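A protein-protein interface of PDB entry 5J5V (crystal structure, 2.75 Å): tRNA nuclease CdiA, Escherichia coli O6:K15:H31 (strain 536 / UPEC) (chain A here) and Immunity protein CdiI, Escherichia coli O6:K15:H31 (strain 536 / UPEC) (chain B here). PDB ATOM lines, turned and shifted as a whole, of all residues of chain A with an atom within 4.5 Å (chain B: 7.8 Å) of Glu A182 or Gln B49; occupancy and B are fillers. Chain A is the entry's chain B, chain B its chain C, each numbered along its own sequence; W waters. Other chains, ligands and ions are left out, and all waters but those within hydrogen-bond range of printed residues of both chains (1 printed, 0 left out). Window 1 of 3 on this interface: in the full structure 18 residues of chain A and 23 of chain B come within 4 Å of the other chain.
NE2 of His A179 sits at hydrogen-bond distance from N of Leu B23. The side-chain amide nitrogen (ND2) of Asn A185 is in hydrogen-bond range of the side-chain carboxylate (OE2) of Glu B77, at 3.3 Å. The backbone carbonyl oxygen of Gln B49 sits at hydrogen-bond distance from the side-chain amino group of Lys A171. OE1 of Glu A182 lies within salt-bridge range of NE of Arg B45. NE2 of Gln B49 sits at hydrogen-bond distance from OE2 of Glu A182 (3.0 Å). The side-chain carboxylate of Glu A182 lies within salt-bridge range of the guanidinium group of Arg B48, 3.0 Å away. The backbone carbonyl oxygen of Asp A178 sits at hydrogen-bond distance from the side-chain amide nitrogen of Gln B49, 3.0 Å away. The backbone carbonyl oxygen of Arg B48 lies close to the side-chain amide oxygen of Gln A181, at 3.1 Å.
OE1 of Glu B41 lies within hydrogen-bond range of OH of Tyr B73 (3.3 Å). The backbone NH (N) of Tyr B73 is in hydrogen-bond range of the side-chain carboxylate (OE1) of Glu B77. The backbone NH of Leu B51 sits at hydrogen-bond distance from the backbone carbonyl oxygen of Ala B46, 3.0 Å away. The side-chain hydroxyl (OG1) of Thr A186 sits at hydrogen-bond distance from the backbone carbonyl oxygen (O) of Glu A182. OD1 of Asp A178 sits at hydrogen-bond distance from N of Gln A181, 2.9 Å away. N of Met A180 lies close to OD1 of Asp A178 (3.4 Å).
NZ of Lys A171 touches CD2 of Leu B51 (3.9 Å). Trp A177 touches Leu B23. Phe B27 touches Trp A177 (CB to CH2, 3.6 Å). Gln B49 touches Trp A177. CH2 of Trp A177 touches CD2 of Leu B51 (3.9 Å). Asp A178 touches Leu B23 (O to CD1, 3.5 Å). CG2 of Thr B84 touches NE2 of Gln A181, at 3.8 Å. Glu A182 touches Leu B23. Arg B48 touches Asn A185 (NH1 to OD1, 3.7 Å). Asn A185 touches Tyr B73 (ND2 to CD2, 3.5 Å).
Of the printed residues of chain B, Trp A177 touches Leu B23, Phe B27, Gln B49 and Leu B51. Printed residues of chain B within 4 Å of Asp A178: Leu B23 and Gln B49. Of the printed residues of chain B, Glu A182 touches Leu B23 (3.99 Å), Arg B45 (3.0 Å), Arg B48 (3.0 Å) and Gln B49 (3.0 Å). Of the printed residues of chain B, Asn A185 touches Arg B48, Tyr B73 and Glu B77. Ile B8 touches none of the printed residues of chain A. The nearest residue of chain A that does not touch Gln B49 is Gln A181 (4.2 Å).
Hydrophobic or aromatic side chains of chain B within 4 Å of the printed part of chain A: Ile B11, Pro B22, Leu B23, Phe B27, Leu B51 and Tyr B73. Along chain B the printed residues that touch a printed residue of chain A span positions 11 to 84.
Water W1 lies within hydrogen-bond range of the guanidinium group (NH1) of Arg B48 (3.0 Å), the backbone carbonyl oxygen (O) of Glu B77 (3.1 Å), the backbone NH (N) of Ala B81 (3.2 Å) and the side-chain amide oxygen (OD1) of Asn A185 (3.3 Å).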
ATOM      1  N   LYS A 171     -14.554 -29.046 -33.943  1.00  0.00           N
ATOM      2  CA  LYS A 171     -14.081 -30.411 -33.817  1.00  0.00           C
ATOM      3  C   LYS A 171     -14.392 -31.192 -35.091  1.00  0.00           C
ATOM      4  O   LYS A 171     -15.140 -30.742 -35.956  1.00  0.00           O
ATOM      5  CB  LYS A 171     -14.726 -31.106 -32.622  1.00  0.00           C
ATOM      6  CG  LYS A 171     -14.576 -30.450 -31.277  1.00  0.00           C
ATOM      7  CD  LYS A 171     -15.521 -31.119 -30.314  1.00  0.00           C
ATOM      8  CE  LYS A 171     -15.410 -30.593 -28.915  1.00  0.00           C
ATOM      9  NZ  LYS A 171     -16.318 -31.315 -27.999  1.00  0.00           N
ATOM     10  N   TRP A 177     -15.098 -26.772 -29.902  1.00  0.00           N
ATOM     11  CA  TRP A 177     -14.516 -26.438 -28.612  1.00  0.00           C
ATOM     12  C   TRP A 177     -15.045 -25.092 -28.150  1.00  0.00           C
ATOM     13  O   TRP A 177     -15.296 -24.195 -28.953  1.00  0.00           O
ATOM     14  CB  TRP A 177     -12.994 -26.391 -28.690  1.00  0.00           C
ATOM     15  CG  TRP A 177     -12.350 -27.661 -29.106  1.00  0.00           C
ATOM     16  CD1 TRP A 177     -11.823 -27.949 -30.325  1.00  0.00           C
ATOM     17  CD2 TRP A 177     -12.136 -28.813 -28.297  1.00  0.00           C
ATOM     18  NE1 TRP A 177     -11.308 -29.212 -30.330  1.00  0.00           N
ATOM     19  CE2 TRP A 177     -11.486 -29.763 -29.091  1.00  0.00           C
ATOM     20  CE3 TRP A 177     -12.438 -29.136 -26.983  1.00  0.00           C
ATOM     21  CZ2 TRP A 177     -11.130 -31.003 -28.611  1.00  0.00           C
ATOM     22  CZ3 TRP A 177     -12.088 -30.365 -26.515  1.00  0.00           C
ATOM     23  CH2 TRP A 177     -11.446 -31.286 -27.323  1.00  0.00           C
ATOM     24  N   ASP A 178     -15.192 -24.950 -26.840  1.00  0.00           N
ATOM     25  CA  ASP A 178     -15.787 -23.766 -26.232  1.00  0.00           C
ATOM     26  C   ASP A 178     -14.744 -23.121 -25.325  1.00  0.00           C
ATOM     27  O   ASP A 178     -14.608 -23.478 -24.156  1.00  0.00           O
ATOM     28  CB  ASP A 178     -17.048 -24.141 -25.460  1.00  0.00           C
ATOM     29  CG  ASP A 178     -17.920 -22.952 -25.145  1.00  0.00           C
ATOM     30  OD1 ASP A 178     -17.384 -21.839 -24.954  1.00  0.00           O
ATOM     31  OD2 ASP A 178     -19.148 -23.143 -25.043  1.00  0.00           O
ATOM     32  N   HIS A 179     -13.997 -22.174 -25.876  1.00  0.00           N
ATOM     33  CA  HIS A 179     -12.979 -21.470 -25.111  1.00  0.00           C
ATOM     34  C   HIS A 179     -13.574 -20.431 -24.172  1.00  0.00           C
ATOM     35  O   HIS A 179     -12.993 -20.155 -23.116  1.00  0.00           O
ATOM     36  CB  HIS A 179     -11.977 -20.831 -26.072  1.00  0.00           C
ATOM     37  CG  HIS A 179     -11.100 -21.829 -26.765  1.00  0.00           C
ATOM     38  ND1 HIS A 179     -11.506 -22.527 -27.881  1.00  0.00           N
ATOM     39  CD2 HIS A 179      -9.853 -22.270 -26.479  1.00  0.00           C
ATOM     40  CE1 HIS A 179     -10.543 -23.347 -28.258  1.00  0.00           C
ATOM     41  NE2 HIS A 179      -9.530 -23.211 -27.424  1.00  0.00           N
ATOM     42  N   MET A 180     -14.712 -19.844 -24.522  1.00  0.00           N
ATOM     43  CA  MET A 180     -15.323 -18.872 -23.635  1.00  0.00           C
ATOM     44  C   MET A 180     -15.966 -19.549 -22.429  1.00  0.00           C
ATOM     45  O   MET A 180     -16.161 -18.918 -21.408  1.00  0.00           O
ATOM     46  CB  MET A 180     -16.352 -18.017 -24.373  1.00  0.00           C
ATOM     47  CG  MET A 180     -17.728 -18.645 -24.517  1.00  0.00           C
ATOM     48  SD  MET A 180     -19.073 -17.366 -25.098  1.00  0.00           S
ATOM     49  CE  MET A 180     -20.076 -17.224 -23.486  1.00  0.00           C
ATOM     50  N   GLN A 181     -16.280 -20.837 -22.518  1.00  0.00           N
ATOM     51  CA  GLN A 181     -16.743 -21.523 -21.318  1.00  0.00           C
ATOM     52  C   GLN A 181     -15.604 -21.733 -20.324  1.00  0.00           C
ATOM     53  O   GLN A 181     -15.806 -21.635 -19.115  1.00  0.00           O
ATOM     54  CB  GLN A 181     -17.404 -22.844 -21.692  1.00  0.00           C
ATOM     55  CG  GLN A 181     -18.058 -23.533 -20.540  1.00  0.00           C
ATOM     56  CD  GLN A 181     -18.693 -24.836 -20.925  1.00  0.00           C
ATOM     57  OE1 GLN A 181     -18.671 -25.232 -22.082  1.00  0.00           O
ATOM     58  NE2 GLN A 181     -19.226 -25.538 -19.941  1.00  0.00           N
ATOM     59  N   GLU A 182     -14.391 -21.989 -20.811  1.00  0.00           N
ATOM     60  CA  GLU A 182     -13.235 -22.049 -19.921  1.00  0.00           C
ATOM     61  C   GLU A 182     -12.956 -20.703 -19.271  1.00  0.00           C
ATOM     62  O   GLU A 182     -12.599 -20.644 -18.094  1.00  0.00           O
ATOM     63  CB  GLU A 182     -12.005 -22.533 -20.678  1.00  0.00           C
ATOM     64  CG  GLU A 182     -12.130 -23.927 -21.221  1.00  0.00           C
ATOM     65  CD  GLU A 182     -12.430 -24.952 -20.139  1.00  0.00           C
ATOM     66  OE1 GLU A 182     -11.686 -25.012 -19.132  1.00  0.00           O
ATOM     67  OE2 GLU A 182     -13.411 -25.703 -20.298  1.00  0.00           O
ATOM     68  N   MET A 183     -13.112 -19.619 -20.013  1.00  0.00           N
ATOM     69  CA  MET A 183     -12.943 -18.289 -19.454  1.00  0.00           C
ATOM     70  C   MET A 183     -13.990 -17.953 -18.411  1.00  0.00           C
ATOM     71  O   MET A 183     -13.680 -17.304 -17.416  1.00  0.00           O
ATOM     72  CB  MET A 183     -12.975 -17.242 -20.556  1.00  0.00           C
ATOM     73  CG  MET A 183     -12.485 -15.871 -20.145  1.00  0.00           C
ATOM     74  SD  MET A 183     -10.765 -15.859 -19.261  1.00  0.00           S
ATOM     75  CE  MET A 183      -9.626 -16.005 -20.767  1.00  0.00           C
ATOM     76  N   GLN A 184     -15.235 -18.394 -18.630  1.00  0.00           N
ATOM     77  CA  GLN A 184     -16.253 -18.201 -17.603  1.00  0.00           C
ATOM     78  C   GLN A 184     -15.898 -18.951 -16.335  1.00  0.00           C
ATOM     79  O   GLN A 184     -16.200 -18.492 -15.236  1.00  0.00           O
ATOM     80  CB  GLN A 184     -17.625 -18.655 -18.073  1.00  0.00           C
ATOM     81  CG  GLN A 184     -18.190 -17.978 -19.291  1.00  0.00           C
ATOM     82  CD  GLN A 184     -19.451 -18.688 -19.729  1.00  0.00           C
ATOM     83  OE1 GLN A 184     -19.844 -18.625 -20.888  1.00  0.00           O
ATOM     84  NE2 GLN A 184     -20.086 -19.383 -18.779  1.00  0.00           N
ATOM     85  N   ASN A 185     -15.322 -20.142 -16.472  1.00  0.00           N
ATOM     86  CA  ASN A 185     -14.911 -20.902 -15.307  1.00  0.00           C
ATOM     87  C   ASN A 185     -13.809 -20.176 -14.554  1.00  0.00           C
ATOM     88  O   ASN A 185     -13.797 -20.161 -13.320  1.00  0.00           O
ATOM     89  CB  ASN A 185     -14.445 -22.285 -15.739  1.00  0.00           C
ATOM     90  CG  ASN A 185     -14.277 -23.224 -14.580  1.00  0.00           C
ATOM     91  OD1 ASN A 185     -15.237 -23.573 -13.909  1.00  0.00           O
ATOM     92  ND2 ASN A 185     -13.053 -23.636 -14.334  1.00  0.00           N
ATOM     93  N   THR A 186     -12.853 -19.602 -15.290  1.00  0.00           N
ATOM     94  CA  THR A 186     -11.752 -18.869 -14.676  1.00  0.00           C
ATOM     95  C   THR A 186     -12.266 -17.646 -13.932  1.00  0.00           C
ATOM     96  O   THR A 186     -11.860 -17.376 -12.797  1.00  0.00           O
ATOM     97  CB  THR A 186     -10.742 -18.470 -15.756  1.00  0.00           C
ATOM     98  OG1 THR A 186     -10.172 -19.647 -16.333  1.00  0.00           O
ATOM     99  CG2 THR A 186      -9.619 -17.635 -15.175  1.00  0.00           C
ATOM    100  N   ILE B   8     -13.545 -42.164 -28.393  1.00  0.00           N
ATOM    101  CA  ILE B   8     -13.958 -41.251 -29.448  1.00  0.00           C
ATOM    102  C   ILE B   8     -12.873 -41.016 -30.478  1.00  0.00           C
ATOM    103  O   ILE B   8     -13.119 -40.314 -31.460  1.00  0.00           O
ATOM    104  CB  ILE B   8     -14.451 -39.909 -28.874  1.00  0.00           C
ATOM    105  CG1 ILE B   8     -13.293 -39.129 -28.251  1.00  0.00           C
ATOM    106  CG2 ILE B   8     -15.542 -40.128 -27.842  1.00  0.00           C
ATOM    107  CD1 ILE B   8     -13.724 -37.805 -27.634  1.00  0.00           C
ATOM    108  N   ILE B  11     -10.754 -36.361 -32.086  1.00  0.00           N
ATOM    109  CA  ILE B  11     -11.774 -35.494 -32.657  1.00  0.00           C
ATOM    110  C   ILE B  11     -11.227 -34.134 -33.038  1.00  0.00           C
ATOM    111  O   ILE B  11     -12.001 -33.253 -33.431  1.00  0.00           O
ATOM    112  CB  ILE B  11     -12.925 -35.293 -31.658  1.00  0.00           C
ATOM    113  CG1 ILE B  11     -12.380 -34.580 -30.429  1.00  0.00           C
ATOM    114  CG2 ILE B  11     -13.531 -36.611 -31.276  1.00  0.00           C
ATOM    115  CD1 ILE B  11     -13.392 -34.305 -29.388  1.00  0.00           C
ATOM    116  N   PRO B  22      -5.781 -23.649 -27.457  1.00  0.00           N
ATOM    117  CA  PRO B  22      -5.514 -24.228 -26.133  1.00  0.00           C
ATOM    118  C   PRO B  22      -6.299 -25.491 -25.819  1.00  0.00           C
ATOM    119  O   PRO B  22      -5.770 -26.382 -25.154  1.00  0.00           O
ATOM    120  CB  PRO B  22      -5.876 -23.078 -25.200  1.00  0.00           C
ATOM    121  CG  PRO B  22      -5.558 -21.892 -25.982  1.00  0.00           C
ATOM    122  CD  PRO B  22      -5.964 -22.192 -27.373  1.00  0.00           C
ATOM    123  N   LEU B  23      -7.537 -25.609 -26.279  1.00  0.00           N
ATOM    124  CA  LEU B  23      -8.306 -26.810 -25.996  1.00  0.00           C
ATOM    125  C   LEU B  23      -7.908 -27.958 -26.914  1.00  0.00           C
ATOM    126  O   LEU B  23      -7.878 -29.117 -26.490  1.00  0.00           O
ATOM    127  CB  LEU B  23      -9.797 -26.496 -26.116  1.00  0.00           C
ATOM    128  CG  LEU B  23     -10.499 -25.742 -24.973  1.00  0.00           C
ATOM    129  CD1 LEU B  23     -11.857 -25.323 -25.394  1.00  0.00           C
ATOM    130  CD2 LEU B  23     -10.597 -26.609 -23.743  1.00  0.00           C
ATOM    131  N   TRP B  26      -4.721 -29.105 -25.313  1.00  0.00           N
ATOM    132  CA  TRP B  26      -5.008 -29.801 -24.067  1.00  0.00           C
ATOM    133  C   TRP B  26      -5.568 -31.186 -24.329  1.00  0.00           C
ATOM    134  O   TRP B  26      -5.206 -32.149 -23.653  1.00  0.00           O
ATOM    135  CB  TRP B  26      -5.980 -28.969 -23.230  1.00  0.00           C
ATOM    136  CG  TRP B  26      -6.638 -29.733 -22.137  1.00  0.00           C
ATOM    137  CD1 TRP B  26      -6.129 -29.984 -20.909  1.00  0.00           C
ATOM    138  CD2 TRP B  26      -7.941 -30.335 -22.164  1.00  0.00           C
ATOM    139  NE1 TRP B  26      -7.020 -30.717 -20.170  1.00  0.00           N
ATOM    140  CE2 TRP B  26      -8.138 -30.949 -20.921  1.00  0.00           C
ATOM    141  CE3 TRP B  26      -8.954 -30.417 -23.122  1.00  0.00           C
ATOM    142  CZ2 TRP B  26      -9.305 -31.633 -20.608  1.00  0.00           C
ATOM    143  CZ3 TRP B  26     -10.110 -31.104 -22.811  1.00  0.00           C
ATOM    144  CH2 TRP B  26     -10.277 -31.697 -21.568  1.00  0.00           C
ATOM    145  N   PHE B  27      -6.436 -31.313 -25.324  1.00  0.00           N
ATOM    146  CA  PHE B  27      -7.035 -32.607 -25.600  1.00  0.00           C
ATOM    147  C   PHE B  27      -5.985 -33.622 -26.034  1.00  0.00           C
ATOM    148  O   PHE B  27      -6.066 -34.796 -25.666  1.00  0.00           O
ATOM    149  CB  PHE B  27      -8.125 -32.445 -26.654  1.00  0.00           C
ATOM    150  CG  PHE B  27      -8.720 -33.739 -27.108  1.00  0.00           C
ATOM    151  CD1 PHE B  27      -9.523 -34.477 -26.268  1.00  0.00           C
ATOM    152  CD2 PHE B  27      -8.477 -34.213 -28.385  1.00  0.00           C
ATOM    153  CE1 PHE B  27     -10.065 -35.677 -26.684  1.00  0.00           C
ATOM    154  CE2 PHE B  27      -9.011 -35.408 -28.810  1.00  0.00           C
ATOM    155  CZ  PHE B  27      -9.807 -36.144 -27.956  1.00  0.00           C
ATOM    156  N   GLU B  41      -8.894 -31.312 -12.444  1.00  0.00           N
ATOM    157  CA  GLU B  41      -8.947 -30.248 -13.438  1.00  0.00           C
ATOM    158  C   GLU B  41      -9.303 -30.801 -14.812  1.00  0.00           C
ATOM    159  O   GLU B  41     -10.163 -30.254 -15.512  1.00  0.00           O
ATOM    160  CB  GLU B  41      -7.604 -29.525 -13.462  1.00  0.00           C
ATOM    161  CG  GLU B  41      -7.489 -28.411 -14.454  1.00  0.00           C
ATOM    162  CD  GLU B  41      -6.076 -27.905 -14.587  1.00  0.00           C
ATOM    163  OE1 GLU B  41      -5.804 -27.153 -15.538  1.00  0.00           O
ATOM    164  OE2 GLU B  41      -5.229 -28.261 -13.746  1.00  0.00           O
ATOM    165  N   ASP B  42      -8.623 -31.873 -15.226  1.00  0.00           N
ATOM    166  CA  ASP B  42      -8.923 -32.514 -16.502  1.00  0.00           C
ATOM    167  C   ASP B  42     -10.349 -33.052 -16.545  1.00  0.00           C
ATOM    168  O   ASP B  42     -11.009 -32.997 -17.586  1.00  0.00           O
ATOM    169  CB  ASP B  42      -7.944 -33.650 -16.761  1.00  0.00           C
ATOM    170  CG  ASP B  42      -6.555 -33.173 -17.085  1.00  0.00           C
ATOM    171  OD1 ASP B  42      -6.378 -32.009 -17.489  1.00  0.00           O
ATOM    172  OD2 ASP B  42      -5.627 -33.990 -16.931  1.00  0.00           O
ATOM    173  N   LEU B  43     -10.828 -33.613 -15.437  1.00  0.00           N
ATOM    174  CA  LEU B  43     -12.169 -34.187 -15.414  1.00  0.00           C
ATOM    175  C   LEU B  43     -13.239 -33.122 -15.635  1.00  0.00           C
ATOM    176  O   LEU B  43     -14.110 -33.272 -16.489  1.00  0.00           O
ATOM    177  CB  LEU B  43     -12.373 -34.923 -14.088  1.00  0.00           C
ATOM    178  CG  LEU B  43     -13.552 -35.876 -13.850  1.00  0.00           C
ATOM    179  CD1 LEU B  43     -13.664 -36.886 -14.938  1.00  0.00           C
ATOM    180  CD2 LEU B  43     -13.392 -36.560 -12.515  1.00  0.00           C
ATOM    181  N   CYS B  44     -13.180 -32.031 -14.884  1.00  0.00           N
ATOM    182  CA  CYS B  44     -14.147 -30.957 -15.074  1.00  0.00           C
ATOM    183  C   CYS B  44     -14.171 -30.481 -16.516  1.00  0.00           C
ATOM    184  O   CYS B  44     -15.240 -30.276 -17.101  1.00  0.00           O
ATOM    185  CB  CYS B  44     -13.815 -29.781 -14.172  1.00  0.00           C
ATOM    186  SG  CYS B  44     -13.898 -30.129 -12.484  1.00  0.00           S
ATOM    187  N   ARG B  45     -12.993 -30.265 -17.095  1.00  0.00           N
ATOM    188  CA  ARG B  45     -12.929 -29.659 -18.413  1.00  0.00           C
ATOM    189  C   ARG B  45     -13.478 -30.606 -19.466  1.00  0.00           C
ATOM    190  O   ARG B  45     -14.211 -30.183 -20.361  1.00  0.00           O
ATOM    191  CB  ARG B  45     -11.483 -29.269 -18.723  1.00  0.00           C
ATOM    192  CG  ARG B  45     -11.275 -28.502 -20.026  1.00  0.00           C
ATOM    193  CD  ARG B  45      -9.859 -27.931 -20.177  1.00  0.00           C
ATOM    194  NE  ARG B  45      -9.472 -26.974 -19.152  1.00  0.00           N
ATOM    195  CZ  ARG B  45      -8.476 -27.164 -18.294  1.00  0.00           C
ATOM    196  NH1 ARG B  45      -7.772 -28.273 -18.346  1.00  0.00           N
ATOM    197  NH2 ARG B  45      -8.187 -26.253 -17.384  1.00  0.00           N
ATOM    198  N   ALA B  46     -13.183 -31.899 -19.343  1.00  0.00           N
ATOM    199  CA  ALA B  46     -13.703 -32.876 -20.288  1.00  0.00           C
ATOM    200  C   ALA B  46     -15.220 -32.922 -20.256  1.00  0.00           C
ATOM    201  O   ALA B  46     -15.863 -33.134 -21.287  1.00  0.00           O
ATOM    202  CB  ALA B  46     -13.120 -34.248 -19.983  1.00  0.00           C
ATOM    203  N   ILE B  47     -15.809 -32.737 -19.076  1.00  0.00           N
ATOM    204  CA  ILE B  47     -17.262 -32.654 -18.959  1.00  0.00           C
ATOM    205  C   ILE B  47     -17.776 -31.396 -19.646  1.00  0.00           C
ATOM    206  O   ILE B  47     -18.617 -31.463 -20.544  1.00  0.00           O
ATOM    207  CB  ILE B  47     -17.681 -32.693 -17.480  1.00  0.00           C
ATOM    208  CG1 ILE B  47     -17.252 -34.009 -16.841  1.00  0.00           C
ATOM    209  CG2 ILE B  47     -19.179 -32.499 -17.342  1.00  0.00           C
ATOM    210  CD1 ILE B  47     -17.471 -34.047 -15.355  1.00  0.00           C
ATOM    211  N   ARG B  48     -17.290 -30.230 -19.215  1.00  0.00           N
ATOM    212  CA  ARG B  48     -17.604 -28.946 -19.837  1.00  0.00           C
ATOM    213  C   ARG B  48     -17.519 -28.985 -21.355  1.00  0.00           C
ATOM    214  O   ARG B  48     -18.305 -28.338 -22.046  1.00  0.00           O
ATOM    215  CB  ARG B  48     -16.670 -27.857 -19.312  1.00  0.00           C
ATOM    216  CG  ARG B  48     -17.015 -27.391 -17.923  1.00  0.00           C
ATOM    217  CD  ARG B  48     -16.418 -26.038 -17.604  1.00  0.00           C
ATOM    218  NE  ARG B  48     -14.965 -26.058 -17.661  1.00  0.00           N
ATOM    219  CZ  ARG B  48     -14.177 -26.436 -16.664  1.00  0.00           C
ATOM    220  NH1 ARG B  48     -14.705 -26.834 -15.521  1.00  0.00           N
ATOM    221  NH2 ARG B  48     -12.860 -26.418 -16.816  1.00  0.00           N
ATOM    222  N   GLN B  49     -16.541 -29.701 -21.882  1.00  0.00           N
ATOM    223  CA  GLN B  49     -16.328 -29.775 -23.316  1.00  0.00           C
ATOM    224  C   GLN B  49     -17.036 -30.954 -23.961  1.00  0.00           C
ATOM    225  O   GLN B  49     -16.803 -31.226 -25.139  1.00  0.00           O
ATOM    226  CB  GLN B  49     -14.826 -29.813 -23.624  1.00  0.00           C
ATOM    227  CG  GLN B  49     -14.092 -28.573 -23.155  1.00  0.00           C
ATOM    228  CD  GLN B  49     -14.625 -27.311 -23.787  1.00  0.00           C
ATOM    229  OE1 GLN B  49     -15.023 -27.314 -24.947  1.00  0.00           O
ATOM    230  NE2 GLN B  49     -14.653 -26.224 -23.021  1.00  0.00           N
ATOM    231  N   ASN B  50     -17.909 -31.635 -23.228  1.00  0.00           N
ATOM    232  CA  ASN B  50     -18.803 -32.634 -23.805  1.00  0.00           C
ATOM    233  C   ASN B  50     -18.009 -33.741 -24.487  1.00  0.00           C
ATOM    234  O   ASN B  50     -18.202 -34.040 -25.664  1.00  0.00           O
ATOM    235  CB  ASN B  50     -19.793 -31.990 -24.781  1.00  0.00           C
ATOM    236  CG  ASN B  50     -20.949 -32.915 -25.138  1.00  0.00           C
ATOM    237  OD1 ASN B  50     -21.529 -33.572 -24.275  1.00  0.00           O
ATOM    238  ND2 ASN B  50     -21.270 -32.991 -26.425  1.00  0.00           N
ATOM    239  N   LEU B  51     -17.083 -34.328 -23.746  1.00  0.00           N
ATOM    240  CA  LEU B  51     -16.185 -35.353 -24.272  1.00  0.00           C
ATOM    241  C   LEU B  51     -16.603 -36.694 -23.686  1.00  0.00           C
ATOM    242  O   LEU B  51     -16.152 -37.068 -22.603  1.00  0.00           O
ATOM    243  CB  LEU B  51     -14.737 -35.060 -23.939  1.00  0.00           C
ATOM    244  CG  LEU B  51     -14.086 -33.789 -24.470  1.00  0.00           C
ATOM    245  CD1 LEU B  51     -12.685 -33.762 -23.957  1.00  0.00           C
ATOM    246  CD2 LEU B  51     -14.105 -33.734 -25.967  1.00  0.00           C
ATOM    247  N   CYS B  52     -17.454 -37.418 -24.420  1.00  0.00           N
ATOM    248  CA  CYS B  52     -18.027 -38.677 -23.954  1.00  0.00           C
ATOM    249  C   CYS B  52     -18.346 -38.643 -22.472  1.00  0.00           C
ATOM    250  O   CYS B  52     -17.756 -39.393 -21.696  1.00  0.00           O
ATOM    251  CB  CYS B  52     -17.094 -39.861 -24.226  1.00  0.00           C
ATOM    252  SG  CYS B  52     -17.988 -41.426 -24.486  1.00  0.00           S
ATOM    253  N   ILE B  53     -19.276 -37.783 -22.066  1.00  0.00           N
ATOM    254  CA  ILE B  53     -19.574 -37.667 -20.644  1.00  0.00           C
ATOM    255  C   ILE B  53     -20.072 -38.992 -20.114  1.00  0.00           C
ATOM    256  O   ILE B  53     -19.834 -39.332 -18.952  1.00  0.00           O
ATOM    257  CB  ILE B  53     -20.603 -36.549 -20.402  1.00  0.00           C
ATOM    258  CG1 ILE B  53     -21.898 -36.893 -21.139  1.00  0.00           C
ATOM    259  CG2 ILE B  53     -20.053 -35.209 -20.841  1.00  0.00           C
ATOM    260  CD1 ILE B  53     -23.137 -36.521 -20.422  1.00  0.00           C
ATOM    261  N   TYR B  73     -10.223 -24.937  -9.779  1.00  0.00           N
ATOM    262  CA  TYR B  73     -10.304 -23.486  -9.777  1.00  0.00           C
ATOM    263  C   TYR B  73     -11.136 -22.949  -8.633  1.00  0.00           C
ATOM    264  O   TYR B  73     -10.934 -21.807  -8.219  1.00  0.00           O
ATOM    265  CB  TYR B  73     -10.875 -23.013 -11.110  1.00  0.00           C
ATOM    266  CG  TYR B  73      -9.932 -23.315 -12.229  1.00  0.00           C
ATOM    267  CD1 TYR B  73      -8.912 -22.431 -12.555  1.00  0.00           C
ATOM    268  CD2 TYR B  73     -10.008 -24.509 -12.916  1.00  0.00           C
ATOM    269  CE1 TYR B  73      -8.016 -22.713 -13.557  1.00  0.00           C
ATOM    270  CE2 TYR B  73      -9.120 -24.803 -13.926  1.00  0.00           C
ATOM    271  CZ  TYR B  73      -8.126 -23.899 -14.240  1.00  0.00           C
ATOM    272  OH  TYR B  73      -7.237 -24.185 -15.238  1.00  0.00           O
ATOM    273  N   GLU B  77     -16.424 -27.151  -8.353  1.00  0.00           N
ATOM    274  CA  GLU B  77     -16.276 -27.020  -9.797  1.00  0.00           C
ATOM    275  C   GLU B  77     -16.799 -28.245 -10.528  1.00  0.00           C
ATOM    276  O   GLU B  77     -17.368 -28.129 -11.618  1.00  0.00           O
ATOM    277  CB  GLU B  77     -14.812 -26.778 -10.156  1.00  0.00           C
ATOM    278  CG  GLU B  77     -14.551 -26.713 -11.647  1.00  0.00           C
ATOM    279  CD  GLU B  77     -13.085 -26.629 -11.970  1.00  0.00           C
ATOM    280  OE1 GLU B  77     -12.282 -26.507 -11.037  1.00  0.00           O
ATOM    281  OE2 GLU B  77     -12.725 -26.744 -13.150  1.00  0.00           O
ATOM    282  N   ALA B  81     -19.466 -28.316 -13.425  1.00  0.00           N
ATOM    283  CA  ALA B  81     -19.320 -28.930 -14.738  1.00  0.00           C
ATOM    284  C   ALA B  81     -20.479 -29.870 -15.039  1.00  0.00           C
ATOM    285  O   ALA B  81     -21.034 -29.847 -16.144  1.00  0.00           O
ATOM    286  CB  ALA B  81     -18.000 -29.687 -14.817  1.00  0.00           C
ATOM    287  N   THR B  84     -23.717 -28.877 -16.638  1.00  0.00           N
ATOM    288  CA  THR B  84     -23.743 -28.568 -18.063  1.00  0.00           C
ATOM    289  C   THR B  84     -24.112 -29.765 -18.920  1.00  0.00           C
ATOM    290  O   THR B  84     -24.176 -29.643 -20.145  1.00  0.00           O
ATOM    291  CB  THR B  84     -22.380 -28.021 -18.499  1.00  0.00           C
ATOM    292  OG1 THR B  84     -21.390 -29.040 -18.343  1.00  0.00           O
ATOM    293  CG2 THR B  84     -21.994 -26.852 -17.633  1.00  0.00           C
HETATM  294  O   HOH W   1     -17.188 -26.198 -14.021  1.00  0.00           O
